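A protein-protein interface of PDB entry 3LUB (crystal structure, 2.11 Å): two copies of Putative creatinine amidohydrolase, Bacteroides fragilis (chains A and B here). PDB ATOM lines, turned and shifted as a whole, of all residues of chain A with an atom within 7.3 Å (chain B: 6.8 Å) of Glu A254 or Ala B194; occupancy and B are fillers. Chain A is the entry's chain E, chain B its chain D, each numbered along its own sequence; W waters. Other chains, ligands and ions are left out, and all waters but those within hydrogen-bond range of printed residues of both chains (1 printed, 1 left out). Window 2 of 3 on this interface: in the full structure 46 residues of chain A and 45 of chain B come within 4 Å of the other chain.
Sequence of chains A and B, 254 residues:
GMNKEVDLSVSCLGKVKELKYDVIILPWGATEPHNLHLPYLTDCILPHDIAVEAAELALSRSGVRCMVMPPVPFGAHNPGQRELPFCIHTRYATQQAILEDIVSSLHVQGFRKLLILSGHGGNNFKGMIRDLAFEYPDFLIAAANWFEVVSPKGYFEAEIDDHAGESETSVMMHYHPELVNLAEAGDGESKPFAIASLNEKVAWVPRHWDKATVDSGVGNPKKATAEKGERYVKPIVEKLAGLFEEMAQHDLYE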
ATOM      1  N   GLU A 246      24.266  16.628 -23.387  1.00  0.00           N
ATOM      2  CA  GLU A 246      24.650  15.228 -23.135  1.00  0.00           C
ATOM      3  C   GLU A 246      25.198  14.574 -24.399  1.00  0.00           C
ATOM      4  O   GLU A 246      26.147  13.803 -24.329  1.00  0.00           O
ATOM      5  CB  GLU A 246      23.478  14.449 -22.584  1.00  0.00           C
ATOM      6  CG  GLU A 246      23.094  14.839 -21.161  1.00  0.00           C
ATOM      7  CD  GLU A 246      21.717  14.354 -20.774  1.00  0.00           C
ATOM      8  OE1 GLU A 246      20.978  13.913 -21.667  1.00  0.00           O
ATOM      9  OE2 GLU A 246      21.368  14.417 -19.572  1.00  0.00           O
ATOM     10  N   GLN A 249      28.672  15.763 -24.607  1.00  0.00           N
ATOM     11  CA  GLN A 249      29.563  15.388 -23.511  1.00  0.00           C
ATOM     12  C   GLN A 249      29.776  13.891 -23.286  1.00  0.00           C
ATOM     13  O   GLN A 249      30.662  13.509 -22.528  1.00  0.00           O
ATOM     14  CB  GLN A 249      29.086  16.085 -22.220  1.00  0.00           C
ATOM     15  CG  GLN A 249      29.232  17.622 -22.347  1.00  0.00           C
ATOM     16  CD  GLN A 249      28.670  18.434 -21.195  1.00  0.00           C
ATOM     17  OE1 GLN A 249      27.766  18.008 -20.476  1.00  0.00           O
ATOM     18  NE2 GLN A 249      29.209  19.645 -21.035  1.00  0.00           N
ATOM     19  N   HIS A 250      28.962  13.059 -23.920  1.00  0.00           N
ATOM     20  CA  HIS A 250      29.032  11.603 -23.762  1.00  0.00           C
ATOM     21  C   HIS A 250      29.048  10.877 -25.112  1.00  0.00           C
ATOM     22  O   HIS A 250      28.437  11.330 -26.080  1.00  0.00           O
ATOM     23  CB  HIS A 250      27.830  11.110 -22.950  1.00  0.00           C
ATOM     24  CG  HIS A 250      27.827  11.589 -21.534  1.00  0.00           C
ATOM     25  ND1 HIS A 250      28.743  11.149 -20.600  1.00  0.00           N
ATOM     26  CD2 HIS A 250      27.029  12.476 -20.893  1.00  0.00           C
ATOM     27  CE1 HIS A 250      28.509  11.752 -19.447  1.00  0.00           C
ATOM     28  NE2 HIS A 250      27.481  12.568 -19.602  1.00  0.00           N
ATOM     29  N   ASP A 251      29.736   9.735 -25.163  1.00  0.00           N
ATOM     30  CA  ASP A 251      29.499   8.769 -26.216  1.00  0.00           C
ATOM     31  C   ASP A 251      28.122   8.166 -25.942  1.00  0.00           C
ATOM     32  O   ASP A 251      27.620   8.265 -24.817  1.00  0.00           O
ATOM     33  CB  ASP A 251      30.596   7.686 -26.270  1.00  0.00           C
ATOM     34  CG  ASP A 251      31.986   8.243 -26.702  1.00  0.00           C
ATOM     35  OD1 ASP A 251      32.050   9.198 -27.524  1.00  0.00           O
ATOM     36  OD2 ASP A 251      33.015   7.720 -26.207  1.00  0.00           O
ATOM     37  N   LEU A 252      27.509   7.597 -26.977  1.00  0.00           N
ATOM     38  CA  LEU A 252      26.199   6.958 -26.869  1.00  0.00           C
ATOM     39  C   LEU A 252      26.169   5.847 -25.805  1.00  0.00           C
ATOM     40  O   LEU A 252      25.157   5.667 -25.073  1.00  0.00           O
ATOM     41  CB  LEU A 252      25.766   6.384 -28.225  1.00  0.00           C
ATOM     42  CG  LEU A 252      24.334   5.852 -28.353  1.00  0.00           C
ATOM     43  CD1 LEU A 252      23.305   6.964 -28.029  1.00  0.00           C
ATOM     44  CD2 LEU A 252      24.142   5.305 -29.758  1.00  0.00           C
ATOM     45  N   TYR A 253      27.256   5.082 -25.759  1.00  0.00           N
ATOM     46  CA  TYR A 253      27.456   4.047 -24.725  1.00  0.00           C
ATOM     47  C   TYR A 253      28.848   4.243 -24.127  1.00  0.00           C
ATOM     48  O   TYR A 253      29.785   4.522 -24.847  1.00  0.00           O
ATOM     49  CB  TYR A 253      27.349   2.633 -25.335  1.00  0.00           C
ATOM     50  CG  TYR A 253      25.951   2.236 -25.797  1.00  0.00           C
ATOM     51  CD1 TYR A 253      25.055   1.647 -24.921  1.00  0.00           C
ATOM     52  CD2 TYR A 253      25.535   2.439 -27.110  1.00  0.00           C
ATOM     53  CE1 TYR A 253      23.785   1.276 -25.333  1.00  0.00           C
ATOM     54  CE2 TYR A 253      24.252   2.083 -27.520  1.00  0.00           C
ATOM     55  CZ  TYR A 253      23.391   1.482 -26.625  1.00  0.00           C
ATOM     56  OH  TYR A 253      22.118   1.077 -26.993  1.00  0.00           O
ATOM     57  N   GLU A 254      28.971   4.110 -22.816  1.00  0.00           N
ATOM     58  CA  GLU A 254      30.278   4.257 -22.142  1.00  0.00           C
ATOM     59  C   GLU A 254      30.552   3.075 -21.233  1.00  0.00           C
ATOM     60  O   GLU A 254      29.671   2.281 -20.958  1.00  0.00           O
ATOM     61  CB  GLU A 254      30.329   5.549 -21.333  1.00  0.00           C
ATOM     62  CG  GLU A 254      30.387   6.762 -22.195  1.00  0.00           C
ATOM     63  CD  GLU A 254      30.257   8.065 -21.422  1.00  0.00           C
ATOM     64  OE1 GLU A 254      29.731   8.077 -20.271  1.00  0.00           O
ATOM     65  OE2 GLU A 254      30.692   9.078 -21.997  1.00  0.00           O
ATOM     66  OXT GLU A 254      31.678   2.891 -20.768  1.00  0.00           O
ATOM     67  N   LYS B 191      21.306  -2.999 -21.403  1.00  0.00           N
ATOM     68  CA  LYS B 191      21.988  -1.852 -20.843  1.00  0.00           C
ATOM     69  C   LYS B 191      21.529  -0.585 -21.533  1.00  0.00           C
ATOM     70  O   LYS B 191      21.328  -0.570 -22.730  1.00  0.00           O
ATOM     71  CB  LYS B 191      23.488  -1.976 -21.007  1.00  0.00           C
ATOM     72  CG  LYS B 191      24.188  -3.066 -20.182  1.00  0.00           C
ATOM     73  CD  LYS B 191      25.690  -3.098 -20.544  1.00  0.00           C
ATOM     74  CE  LYS B 191      26.591  -3.685 -19.456  1.00  0.00           C
ATOM     75  NZ  LYS B 191      28.011  -3.164 -19.595  1.00  0.00           N
ATOM     76  N   PRO B 192      21.370   0.494 -20.776  1.00  0.00           N
ATOM     77  CA  PRO B 192      20.905   1.725 -21.337  1.00  0.00           C
ATOM     78  C   PRO B 192      22.009   2.532 -22.027  1.00  0.00           C
ATOM     79  O   PRO B 192      23.190   2.174 -22.005  1.00  0.00           O
ATOM     80  CB  PRO B 192      20.439   2.488 -20.099  1.00  0.00           C
ATOM     81  CG  PRO B 192      21.409   2.086 -19.051  1.00  0.00           C
ATOM     82  CD  PRO B 192      21.630   0.622 -19.326  1.00  0.00           C
ATOM     83  N   PHE B 193      21.595   3.652 -22.598  1.00  0.00           N
ATOM     84  CA  PHE B 193      22.515   4.631 -23.143  1.00  0.00           C
ATOM     85  C   PHE B 193      23.262   5.395 -22.039  1.00  0.00           C
ATOM     86  O   PHE B 193      22.816   5.472 -20.884  1.00  0.00           O
ATOM     87  CB  PHE B 193      21.762   5.673 -23.979  1.00  0.00           C
ATOM     88  CG  PHE B 193      21.068   5.126 -25.198  1.00  0.00           C
ATOM     89  CD1 PHE B 193      21.794   4.512 -26.235  1.00  0.00           C
ATOM     90  CD2 PHE B 193      19.688   5.309 -25.358  1.00  0.00           C
ATOM     91  CE1 PHE B 193      21.138   4.050 -27.387  1.00  0.00           C
ATOM     92  CE2 PHE B 193      19.029   4.863 -26.509  1.00  0.00           C
ATOM     93  CZ  PHE B 193      19.750   4.230 -27.534  1.00  0.00           C
ATOM     94  N   ALA B 194      24.382   5.998 -22.433  1.00  0.00           N
ATOM     95  CA  ALA B 194      25.115   6.925 -21.582  1.00  0.00           C
ATOM     96  C   ALA B 194      24.535   8.328 -21.638  1.00  0.00           C
ATOM     97  O   ALA B 194      24.965   9.204 -20.892  1.00  0.00           O
ATOM     98  CB  ALA B 194      26.584   6.971 -21.987  1.00  0.00           C
ATOM     99  N   ILE B 195      23.578   8.549 -22.538  1.00  0.00           N
ATOM    100  CA  ILE B 195      22.951   9.851 -22.738  1.00  0.00           C
ATOM    101  C   ILE B 195      21.573   9.752 -22.117  1.00  0.00           C
ATOM    102  O   ILE B 195      20.656   9.125 -22.674  1.00  0.00           O
ATOM    103  CB  ILE B 195      22.950  10.225 -24.244  1.00  0.00           C
ATOM    104  CG1 ILE B 195      24.386  10.410 -24.733  1.00  0.00           C
ATOM    105  CG2 ILE B 195      22.144  11.483 -24.522  1.00  0.00           C
ATOM    106  CD1 ILE B 195      24.560  10.377 -26.299  1.00  0.00           C
ATOM    107  N   ALA B 196      21.456  10.348 -20.924  1.00  0.00           N
ATOM    108  CA  ALA B 196      20.298  10.220 -20.072  1.00  0.00           C
ATOM    109  C   ALA B 196      19.042  10.614 -20.810  1.00  0.00           C
ATOM    110  O   ALA B 196      18.052   9.936 -20.691  1.00  0.00           O
ATOM    111  CB  ALA B 196      20.495  11.077 -18.809  1.00  0.00           C
ATOM    112  N   SER B 197      19.075  11.723 -21.560  1.00  0.00           N
ATOM    113  CA  SER B 197      17.883  12.197 -22.309  1.00  0.00           C
ATOM    114  C   SER B 197      17.378  11.193 -23.348  1.00  0.00           C
ATOM    115  O   SER B 197      16.205  11.178 -23.674  1.00  0.00           O
ATOM    116  CB  SER B 197      18.183  13.555 -22.992  1.00  0.00           C
ATOM    117  OG  SER B 197      18.508  14.572 -22.043  1.00  0.00           O
ATOM    118  N   ASN B 199      17.536   7.803 -22.843  1.00  0.00           N
ATOM    119  CA  ASN B 199      16.802   6.857 -21.966  1.00  0.00           C
ATOM    120  C   ASN B 199      15.438   7.429 -21.524  1.00  0.00           C
ATOM    121  O   ASN B 199      14.479   6.684 -21.345  1.00  0.00           O
ATOM    122  CB  ASN B 199      17.641   6.457 -20.738  1.00  0.00           C
ATOM    123  CG  ASN B 199      18.975   5.824 -21.106  1.00  0.00           C
ATOM    124  OD1 ASN B 199      19.061   4.990 -22.008  1.00  0.00           O
ATOM    125  ND2 ASN B 199      20.030   6.226 -20.410  1.00  0.00           N
ATOM    126  N   LYS B 211      26.112  -3.308 -27.722  1.00  0.00           N
ATOM    127  CA  LYS B 211      26.403  -2.668 -26.428  1.00  0.00           C
ATOM    128  C   LYS B 211      25.302  -2.864 -25.386  1.00  0.00           C
ATOM    129  O   LYS B 211      25.553  -2.841 -24.179  1.00  0.00           O
ATOM    130  CB  LYS B 211      26.603  -1.182 -26.631  1.00  0.00           C
ATOM    131  CG  LYS B 211      27.544  -0.801 -27.761  1.00  0.00           C
ATOM    132  CD  LYS B 211      28.982  -0.910 -27.350  1.00  0.00           C
ATOM    133  CE  LYS B 211      29.879  -0.093 -28.254  1.00  0.00           C
ATOM    134  NZ  LYS B 211      29.586  -0.330 -29.688  1.00  0.00           N
HETATM  135  O   HOH W   1      20.485   0.712 -25.055  1.00  0.00           O
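The backbone carbonyl oxygen (O) of Leu A252 is in hydrogen-bond range of the backbone NH (N) of Ala B194. The side-chain hydroxyl of Ser B197 lies within hydrogen-bond range of the side-chain carboxylate of Glu A246 (2.6 Å).
O of Phe B193 lies within hydrogen-bond range of ND2 of Asn B199 (2.9 Å). OE2 of Glu A254 sits at hydrogen-bond distance from ND1 of His A250. The backbone NH (N) of Asp A251 is in hydrogen-bond range of the side-chain carboxylate (OE2) of Glu A254.
Glu A254 touches just one residue of chain B: Ala B194. Of chain A, only His A250 (3.8 Å), Asp A251 (3.3 Å), Leu A252 (2.8 Å) and Glu A254 (3.8 Å) come within 4 Å of Ala B194. Of the printed residues of chain B, Glu A246 touches Ile B195 (3.8 Å), Ala B196 (3.5 Å) and Ser B197 (2.6 Å). Of the printed residues of chain A, Lys B211 touches Tyr A253 (3.6 Å). Printed residues of chain B within 4 Å of His A250: Ala B194 and Ile B195. Asn B199 touches none of the printed residues of chain A. The nearest residue of chain B that does not touch Glu A254 is Lys B191 (5.9 Å). The nearest residue of chain A that does not touch Ala B194 is Tyr A253 (4.1 Å).
Hydrophobic or aromatic side chains of chain B that line the printed part of chain A: Phe B193, Ala B194, Ile B195 and Ala B196. Hydrophobic or aromatic side chains of chain A within 4 Å of the printed part of chain B: His A250, Leu A252 and Tyr A253. Along chain A the printed residues that touch a printed residue of chain B span positions 246 to 254. Among the printed residues, 14 pairs touch across the chains.
Water W1 lies within hydrogen-bond range of the side-chain hydroxyl (OH) of Tyr A253 (2.6 Å) and the backbone carbonyl oxygen (O) of Lys B191 (2.8 Å).
His A250 touches Ala B194. CB of His A250 touches CG1 of Ile B195 (3.9 Å). Asp A251 touches Ala B194 (O to CB, 3.3 Å). Asp A251 touches Ile B195. Leu A252 touches Phe B193. Leu A252 touches Ile B195. O of Pro B192 touches CE1 of Tyr A253, at 3.5 Å. CE1 of Phe B193 touches OH of Tyr A253, at 3.2 Å. Tyr A253 touches Lys B211. OE1 of Glu A254 touches CB of Ala B194 (3.8 Å).
No position is printed for both chains. Of the 14 pairs that touch across the chains among the printed residues, none has its exchanged pair printed and touching as well.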
